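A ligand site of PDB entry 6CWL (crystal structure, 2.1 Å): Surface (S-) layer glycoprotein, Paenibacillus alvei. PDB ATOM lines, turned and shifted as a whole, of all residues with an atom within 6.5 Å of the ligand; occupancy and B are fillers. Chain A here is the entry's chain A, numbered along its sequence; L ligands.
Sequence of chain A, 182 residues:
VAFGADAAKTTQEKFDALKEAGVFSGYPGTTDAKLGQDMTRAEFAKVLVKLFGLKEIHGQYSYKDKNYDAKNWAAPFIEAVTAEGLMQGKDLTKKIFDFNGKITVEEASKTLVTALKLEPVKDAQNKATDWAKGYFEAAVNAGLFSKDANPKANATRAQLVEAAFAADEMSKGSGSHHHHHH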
ATOM      1  N   ARG A  41      33.708  -5.155  -7.155  1.00  0.00           N
ATOM      2  CA  ARG A  41      32.504  -5.289  -6.405  1.00  0.00           C
ATOM      3  C   ARG A  41      31.536  -4.136  -6.702  1.00  0.00           C
ATOM      4  O   ARG A  41      30.353  -4.346  -6.728  1.00  0.00           O
ATOM      5  CB  ARG A  41      32.745  -5.478  -4.910  1.00  0.00           C
ATOM      6  CG  ARG A  41      33.494  -6.781  -4.585  1.00  0.00           C
ATOM      7  CD  ARG A  41      34.182  -6.731  -3.226  1.00  0.00           C
ATOM      8  NE  ARG A  41      33.297  -6.276  -2.120  1.00  0.00           N
ATOM      9  CZ  ARG A  41      32.380  -7.026  -1.523  1.00  0.00           C
ATOM     10  NH1 ARG A  41      32.143  -8.258  -1.927  1.00  0.00           N
ATOM     11  NH2 ARG A  41      31.645  -6.522  -0.549  1.00  0.00           N
ATOM     12  N   TYR A  63      28.521   3.262   3.906  1.00  0.00           N
ATOM     13  CA  TYR A  63      29.891   2.780   4.085  1.00  0.00           C
ATOM     14  C   TYR A  63      30.931   3.909   4.171  1.00  0.00           C
ATOM     15  O   TYR A  63      30.722   5.026   3.711  1.00  0.00           O
ATOM     16  CB  TYR A  63      30.277   1.822   2.959  1.00  0.00           C
ATOM     17  CG  TYR A  63      29.333   0.645   2.825  1.00  0.00           C
ATOM     18  CD1 TYR A  63      29.443  -0.463   3.680  1.00  0.00           C
ATOM     19  CD2 TYR A  63      28.345   0.612   1.811  1.00  0.00           C
ATOM     20  CE1 TYR A  63      28.601  -1.569   3.540  1.00  0.00           C
ATOM     21  CE2 TYR A  63      27.466  -0.465   1.705  1.00  0.00           C
ATOM     22  CZ  TYR A  63      27.596  -1.565   2.558  1.00  0.00           C
ATOM     23  OH  TYR A  63      26.775  -2.674   2.425  1.00  0.00           O
ATOM     24  N   LEU A  86      21.375  -8.070  -0.334  1.00  0.00           N
ATOM     25  CA  LEU A  86      22.206  -8.990  -1.134  1.00  0.00           C
ATOM     26  C   LEU A  86      23.658  -8.950  -0.715  1.00  0.00           C
ATOM     27  O   LEU A  86      24.379  -9.934  -0.888  1.00  0.00           O
ATOM     28  CB  LEU A  86      22.095  -8.655  -2.603  1.00  0.00           C
ATOM     29  CG  LEU A  86      20.682  -8.698  -3.169  1.00  0.00           C
ATOM     30  CD1 LEU A  86      20.732  -8.332  -4.640  1.00  0.00           C
ATOM     31  CD2 LEU A  86      20.029 -10.047  -2.989  1.00  0.00           C
ATOM     32  N   MET A  87      24.128  -7.801  -0.272  1.00  0.00           N
ATOM     33  CA  MET A  87      25.487  -7.604   0.116  1.00  0.00           C
ATOM     34  C   MET A  87      25.558  -6.718   1.342  1.00  0.00           C
ATOM     35  O   MET A  87      24.819  -5.740   1.454  1.00  0.00           O
ATOM     36  CB  MET A  87      26.280  -6.957  -1.024  1.00  0.00           C
ATOM     37  CG  MET A  87      26.212  -7.701  -2.387  1.00  0.00           C
ATOM     38  SD  MET A  87      27.228  -6.880  -3.646  1.00  0.00           S
ATOM     39  CE  MET A  87      28.870  -7.401  -3.117  1.00  0.00           C
ATOM     40  N   GLN A  88      26.447  -7.022   2.268  1.00  0.00           N
ATOM     41  CA  GLN A  88      26.636  -6.154   3.447  1.00  0.00           C
ATOM     42  C   GLN A  88      28.068  -5.669   3.702  1.00  0.00           C
ATOM     43  O   GLN A  88      28.344  -4.989   4.679  1.00  0.00           O
ATOM     44  CB  GLN A  88      25.898  -6.663   4.692  1.00  0.00           C
ATOM     45  CG  GLN A  88      25.655  -8.141   4.773  1.00  0.00           C
ATOM     46  CD  GLN A  88      26.667  -8.848   5.660  1.00  0.00           C
ATOM     47  OE1 GLN A  88      27.811  -8.388   5.829  1.00  0.00           O
ATOM     48  NE2 GLN A  88      26.263  -9.968   6.243  1.00  0.00           N
ATOM     49  N   GLY A  89      28.955  -5.901   2.749  1.00  0.00           N
ATOM     50  CA  GLY A  89      30.339  -5.454   2.906  1.00  0.00           C
ATOM     51  C   GLY A  89      31.183  -6.460   3.696  1.00  0.00           C
ATOM     52  O   GLY A  89      30.749  -7.566   4.035  1.00  0.00           O
ATOM     53  N   LYS A  90      32.399  -6.049   4.013  1.00  0.00           N
ATOM     54  CA  LYS A  90      33.425  -6.970   4.538  1.00  0.00           C
ATOM     55  C   LYS A  90      33.687  -6.818   6.029  1.00  0.00           C
ATOM     56  O   LYS A  90      34.167  -7.737   6.650  1.00  0.00           O
ATOM     57  CB  LYS A  90      34.719  -6.789   3.774  1.00  0.00           C
ATOM     58  CG  LYS A  90      34.559  -7.203   2.332  1.00  0.00           C
ATOM     59  CD  LYS A  90      35.920  -7.331   1.662  1.00  0.00           C
ATOM     60  CE  LYS A  90      35.800  -8.204   0.432  1.00  0.00           C
ATOM     61  NZ  LYS A  90      36.961  -7.902  -0.426  1.00  0.00           N
ATOM     62  N   ASP A  91      33.364  -5.666   6.608  1.00  0.00           N
ATOM     63  CA  ASP A  91      33.275  -5.585   8.070  1.00  0.00           C
ATOM     64  C   ASP A  91      32.421  -4.444   8.585  1.00  0.00           C
ATOM     65  O   ASP A  91      32.513  -3.234   8.225  1.00  0.00           O
ATOM     66  CB  ASP A  91      34.623  -5.634   8.792  1.00  0.00           C
ATOM     67  CG  ASP A  91      35.458  -4.428   8.526  1.00  0.00           C
ATOM     68  OD1 ASP A  91      35.365  -3.962   7.363  1.00  0.00           O
ATOM     69  OD2 ASP A  91      36.189  -3.989   9.457  1.00  0.00           O
ATOM     70  N   LEU A  92      31.579  -4.902   9.479  1.00  0.00           N
ATOM     71  CA  LEU A  92      30.420  -4.166   9.854  1.00  0.00           C
ATOM     72  C   LEU A  92      30.915  -3.035  10.722  1.00  0.00           C
ATOM     73  O   LEU A  92      30.522  -1.908  10.530  1.00  0.00           O
ATOM     74  CB  LEU A  92      29.440  -5.103  10.581  1.00  0.00           C
ATOM     75  CG  LEU A  92      29.147  -6.415   9.833  1.00  0.00           C
ATOM     76  CD1 LEU A  92      28.244  -7.314  10.670  1.00  0.00           C
ATOM     77  CD2 LEU A  92      28.524  -6.140   8.461  1.00  0.00           C
ATOM     78  N   PHE A  97      33.001  -1.567   2.454  1.00  0.00           N
ATOM     79  CA  PHE A  97      32.358  -2.410   1.460  1.00  0.00           C
ATOM     80  C   PHE A  97      33.418  -3.069   0.589  1.00  0.00           C
ATOM     81  O   PHE A  97      33.200  -4.164   0.127  1.00  0.00           O
ATOM     82  CB  PHE A  97      31.391  -1.600   0.563  1.00  0.00           C
ATOM     83  CG  PHE A  97      30.642  -2.430  -0.435  1.00  0.00           C
ATOM     84  CD1 PHE A  97      29.596  -3.248  -0.046  1.00  0.00           C
ATOM     85  CD2 PHE A  97      30.988  -2.402  -1.788  1.00  0.00           C
ATOM     86  CE1 PHE A  97      28.891  -3.987  -0.960  1.00  0.00           C
ATOM     87  CE2 PHE A  97      30.284  -3.174  -2.729  1.00  0.00           C
ATOM     88  CZ  PHE A  97      29.230  -3.974  -2.307  1.00  0.00           C
ATOM     89  N   ILE A 103      35.128  -8.960  -7.129  1.00  0.00           N
ATOM     90  CA  ILE A 103      34.135  -9.940  -6.691  1.00  0.00           C
ATOM     91  C   ILE A 103      34.676 -11.379  -6.871  1.00  0.00           C
ATOM     92  O   ILE A 103      35.231 -11.726  -7.971  1.00  0.00           O
ATOM     93  CB  ILE A 103      32.788  -9.773  -7.438  1.00  0.00           C
ATOM     94  CG1 ILE A 103      31.702 -10.653  -6.814  1.00  0.00           C
ATOM     95  CG2 ILE A 103      32.845 -10.123  -8.910  1.00  0.00           C
ATOM     96  CD1 ILE A 103      31.037  -9.964  -5.625  1.00  0.00           C
ATOM     97  N   THR A 104      34.488 -12.198  -5.841  1.00  0.00           N
ATOM     98  CA  THR A 104      34.899 -13.605  -5.848  1.00  0.00           C
ATOM     99  C   THR A 104      33.699 -14.502  -6.202  1.00  0.00           C
ATOM    100  O   THR A 104      32.531 -14.075  -6.157  1.00  0.00           O
ATOM    101  CB  THR A 104      35.465 -14.073  -4.494  1.00  0.00           C
ATOM    102  OG1 THR A 104      34.436 -14.026  -3.502  1.00  0.00           O
ATOM    103  CG2 THR A 104      36.677 -13.237  -4.059  1.00  0.00           C
ATOM    104  N   GLU A 106      32.576 -17.203  -4.629  1.00  0.00           N
ATOM    105  CA  GLU A 106      31.717 -17.425  -3.468  1.00  0.00           C
ATOM    106  C   GLU A 106      30.862 -16.152  -3.126  1.00  0.00           C
ATOM    107  O   GLU A 106      29.716 -16.280  -2.740  1.00  0.00           O
ATOM    108  CB  GLU A 106      32.481 -17.900  -2.280  1.00  0.00           C
ATOM    109  CG  GLU A 106      33.557 -16.957  -1.781  1.00  0.00           C
ATOM    110  CD  GLU A 106      34.367 -17.595  -0.666  1.00  0.00           C
ATOM    111  OE1 GLU A 106      34.416 -18.842  -0.585  1.00  0.00           O
ATOM    112  OE2 GLU A 106      34.924 -16.846   0.153  1.00  0.00           O
ATOM    113  N   GLU A 107      31.426 -14.957  -3.254  1.00  0.00           N
ATOM    114  CA  GLU A 107      30.667 -13.711  -2.979  1.00  0.00           C
ATOM    115  C   GLU A 107      29.493 -13.558  -3.966  1.00  0.00           C
ATOM    116  O   GLU A 107      28.375 -13.246  -3.577  1.00  0.00           O
ATOM    117  CB  GLU A 107      31.577 -12.489  -3.054  1.00  0.00           C
ATOM    118  CG  GLU A 107      32.565 -12.310  -1.867  1.00  0.00           C
ATOM    119  CD  GLU A 107      33.565 -11.211  -2.155  1.00  0.00           C
ATOM    120  OE1 GLU A 107      33.469 -10.577  -3.218  1.00  0.00           O
ATOM    121  OE2 GLU A 107      34.465 -10.909  -1.313  1.00  0.00           O
ATOM    122  N   ALA A 108      29.785 -13.767  -5.246  1.00  0.00           N
ATOM    123  CA  ALA A 108      28.792 -13.758  -6.287  1.00  0.00           C
ATOM    124  C   ALA A 108      27.702 -14.795  -6.033  1.00  0.00           C
ATOM    125  O   ALA A 108      26.512 -14.491  -6.154  1.00  0.00           O
ATOM    126  CB  ALA A 108      29.430 -13.994  -7.630  1.00  0.00           C
ATOM    127  N   LYS A 110      26.688 -16.017  -3.150  1.00  0.00           N
ATOM    128  CA  LYS A 110      25.827 -15.584  -2.082  1.00  0.00           C
ATOM    129  C   LYS A 110      24.753 -14.618  -2.618  1.00  0.00           C
ATOM    130  O   LYS A 110      23.570 -14.737  -2.287  1.00  0.00           O
ATOM    131  CB  LYS A 110      26.654 -14.875  -1.022  1.00  0.00           C
ATOM    132  CG  LYS A 110      25.819 -14.607   0.213  1.00  0.00           C
ATOM    133  CD  LYS A 110      25.773 -13.163   0.635  1.00  0.00           C
ATOM    134  CE  LYS A 110      24.356 -12.957   1.147  1.00  0.00           C
ATOM    135  NZ  LYS A 110      24.232 -11.655   1.830  1.00  0.00           N
ATOM    136  N   THR A 111      25.167 -13.683  -3.441  1.00  0.00           N
ATOM    137  CA  THR A 111      24.245 -12.606  -3.862  1.00  0.00           C
ATOM    138  C   THR A 111      23.166 -13.159  -4.763  1.00  0.00           C
ATOM    139  O   THR A 111      22.000 -12.731  -4.696  1.00  0.00           O
ATOM    140  CB  THR A 111      24.965 -11.469  -4.587  1.00  0.00           C
ATOM    141  OG1 THR A 111      25.502 -11.960  -5.813  1.00  0.00           O
ATOM    142  CG2 THR A 111      26.047 -10.883  -3.723  1.00  0.00           C
ATOM    143  N   THR A 114      20.744 -15.659  -2.819  1.00  0.00           N
ATOM    144  CA  THR A 114      19.868 -14.799  -2.023  1.00  0.00           C
ATOM    145  C   THR A 114      18.808 -14.143  -2.913  1.00  0.00           C
ATOM    146  O   THR A 114      17.636 -14.226  -2.615  1.00  0.00           O
ATOM    147  CB  THR A 114      20.695 -13.709  -1.311  1.00  0.00           C
ATOM    148  OG1 THR A 114      21.688 -14.347  -0.496  1.00  0.00           O
ATOM    149  CG2 THR A 114      19.813 -12.810  -0.425  1.00  0.00           C
ATOM    150  N   TRP A 131      32.088 -19.196   5.955  1.00  0.00           N
ATOM    151  CA  TRP A 131      30.824 -18.448   5.801  1.00  0.00           C
ATOM    152  C   TRP A 131      30.067 -18.730   4.488  1.00  0.00           C
ATOM    153  O   TRP A 131      28.849 -18.599   4.426  1.00  0.00           O
ATOM    154  CB  TRP A 131      31.047 -16.929   5.976  1.00  0.00           C
ATOM    155  CG  TRP A 131      31.853 -16.192   4.887  1.00  0.00           C
ATOM    156  CD1 TRP A 131      33.170 -15.781   4.961  1.00  0.00           C
ATOM    157  CD2 TRP A 131      31.368 -15.726   3.616  1.00  0.00           C
ATOM    158  NE1 TRP A 131      33.536 -15.128   3.819  1.00  0.00           N
ATOM    159  CE2 TRP A 131      32.448 -15.073   2.965  1.00  0.00           C
ATOM    160  CE3 TRP A 131      30.129 -15.807   2.945  1.00  0.00           C
ATOM    161  CZ2 TRP A 131      32.336 -14.516   1.681  1.00  0.00           C
ATOM    162  CZ3 TRP A 131      30.005 -15.244   1.656  1.00  0.00           C
ATOM    163  CH2 TRP A 131      31.101 -14.596   1.054  1.00  0.00           C
ATOM    164  N   ALA A 132      30.796 -19.149   3.449  1.00  0.00           N
ATOM    165  CA  ALA A 132      30.241 -19.256   2.096  1.00  0.00           C
ATOM    166  C   ALA A 132      29.881 -20.642   1.635  1.00  0.00           C
ATOM    167  O   ALA A 132      29.212 -20.765   0.625  1.00  0.00           O
ATOM    168  CB  ALA A 132      31.233 -18.674   1.114  1.00  0.00           C
ATOM    169  N   TYR A 135      26.446 -21.263   0.470  1.00  0.00           N
ATOM    170  CA  TYR A 135      26.015 -20.489  -0.660  1.00  0.00           C
ATOM    171  C   TYR A 135      26.669 -20.976  -1.950  1.00  0.00           C
ATOM    172  O   TYR A 135      25.983 -21.117  -2.958  1.00  0.00           O
ATOM    173  CB  TYR A 135      26.214 -19.000  -0.455  1.00  0.00           C
ATOM    174  CG  TYR A 135      25.194 -18.402   0.486  1.00  0.00           C
ATOM    175  CD1 TYR A 135      23.889 -18.116   0.052  1.00  0.00           C
ATOM    176  CD2 TYR A 135      25.526 -18.091   1.801  1.00  0.00           C
ATOM    177  CE1 TYR A 135      22.963 -17.523   0.907  1.00  0.00           C
ATOM    178  CE2 TYR A 135      24.602 -17.530   2.652  1.00  0.00           C
ATOM    179  CZ  TYR A 135      23.329 -17.253   2.207  1.00  0.00           C
ATOM    180  OH  TYR A 135      22.431 -16.681   3.069  1.00  0.00           O
HETATM  181  C1  LIG L   1      31.205  -8.518   7.443  1.00  0.00           C
HETATM  182  C2  LIG L   1      31.570  -9.902   6.919  1.00  0.00           C
HETATM  183  O1  LIG L   1      31.729 -10.830   7.713  1.00  0.00           O
HETATM  184  N1  LIG L   1      31.668 -10.024   5.583  1.00  0.00           N
HETATM  185  C3  LIG L   1      31.969 -11.313   4.933  1.00  0.00           C
HETATM  186  C4  LIG L   1      33.214 -11.216   4.170  1.00  0.00           C
HETATM  187  O2  LIG L   1      34.288 -10.934   5.082  1.00  0.00           O
HETATM  188  C5  LIG L   1      35.579 -10.971   4.443  1.00  0.00           C
HETATM  189  O3  LIG L   1      33.065 -10.195   3.158  1.00  0.00           O
HETATM  190  C6  LIG L   1      32.096 -10.617   2.177  1.00  0.00           C
HETATM  191  C7  LIG L   1      32.010  -9.593   1.092  1.00  0.00           C
HETATM  192  O4  LIG L   1      30.993 -10.023   0.125  1.00  0.00           O
HETATM  193  C8  LIG L   1      29.703 -10.305   0.639  1.00  0.00           C
HETATM  194  C9  LIG L   1      28.847 -11.025  -0.424  1.00  0.00           C
HETATM  195  C10 LIG L   1      29.020  -8.934   1.004  1.00  0.00           C
HETATM  196  O5  LIG L   1      29.464  -7.854   0.525  1.00  0.00           O
HETATM  197  O6  LIG L   1      28.077  -9.021   1.747  1.00  0.00           O
HETATM  198  O7  LIG L   1      29.800 -11.219   1.788  1.00  0.00           O
HETATM  199  C11 LIG L   1      30.750 -10.751   2.802  1.00  0.00           C
HETATM  200  C12 LIG L   1      30.821 -11.677   4.025  1.00  0.00           C
HETATM  201  O8  LIG L   1      29.638 -11.493   4.822  1.00  0.00           O
HETATM  202  C13 LIG L   1      29.294 -12.666   5.504  1.00  0.00           C
HETATM  203  O9  LIG L   1      28.240 -12.963   4.641  1.00  0.00           O
HETATM  204  C14 LIG L   1      27.592 -14.120   5.045  1.00  0.00           C
HETATM  205  C15 LIG L   1      26.736 -14.592   3.893  1.00  0.00           C
HETATM  206  O10 LIG L   1      25.377 -14.200   4.154  1.00  0.00           O
HETATM  207  C16 LIG L   1      26.791 -13.785   6.249  1.00  0.00           C
HETATM  208  O11 LIG L   1      26.066 -14.939   6.615  1.00  0.00           O
HETATM  209  C17 LIG L   1      27.747 -13.402   7.380  1.00  0.00           C
HETATM  210  O12 LIG L   1      26.999 -12.808   8.439  1.00  0.00           O
HETATM  211  C18 LIG L   1      28.798 -12.378   6.928  1.00  0.00           C
HETATM  212  N2  LIG L   1      29.871 -12.312   7.956  1.00  0.00           N
HETATM  213  C19 LIG L   1      30.652 -13.357   8.299  1.00  0.00           C
HETATM  214  O13 LIG L   1      30.607 -14.448   7.749  1.00  0.00           O
HETATM  215  C20 LIG L   1      31.652 -13.107   9.447  1.00  0.00           C
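An oxygen (O6) of the ligand is in hydrogen-bond range of the backbone NH (N) of Gln 88 (2.6 Å).
An oxygen (O5) of the ligand is in salt-bridge range of the guanidinium group (NH2) of Arg 41, 2.8 Å away.
The backbone NH (N) of Gly 89 sits at hydrogen-bond distance from an oxygen (O5) of the ligand, at 3.0 Å.
The backbone carbonyl oxygen of Gly 89 lies within hydrogen-bond range of a nitrogen (N1) of the ligand (3.0 Å).
NH1 of Arg 41 lies within salt-bridge range of OE1 of Glu 107.
O of Phe 97 sits at hydrogen-bond distance from NH2 of Arg 41, 2.9 Å away.
The backbone carbonyl oxygen (O) of Leu 86 is in hydrogen-bond range of the side-chain amino group (NZ) of Lys 110.
The backbone carbonyl oxygen (O) of Lys 110 sits at hydrogen-bond distance from the side-chain hydroxyl (OG1) of Thr 114 (2.6 Å).
The side-chain hydroxyl (OG1) of Thr 104 sits close to the backbone NH (N) of Glu 107.
Met 87 touches the ligand (CA to O6, 3.4 Å).
O of Lys 90 touches C1 of the ligand, at 3.2 Å.
CA of Asp 91 touches C1 of the ligand, at 3.6 Å.
Leu 92 touches the ligand.
Glu 107 touches the ligand.
Lys 110 touches the ligand (CE to O10, 3.4 Å).
Trp 131 touches the ligand.
Tyr 135 touches the ligand (CE2 to O10, 3.7 Å).
Along chain A the residues within 4 Å of the ligand span positions 41 to 135.
The nearest printed residue that does not touch the ligand is Phe 97 (4.2 Å).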
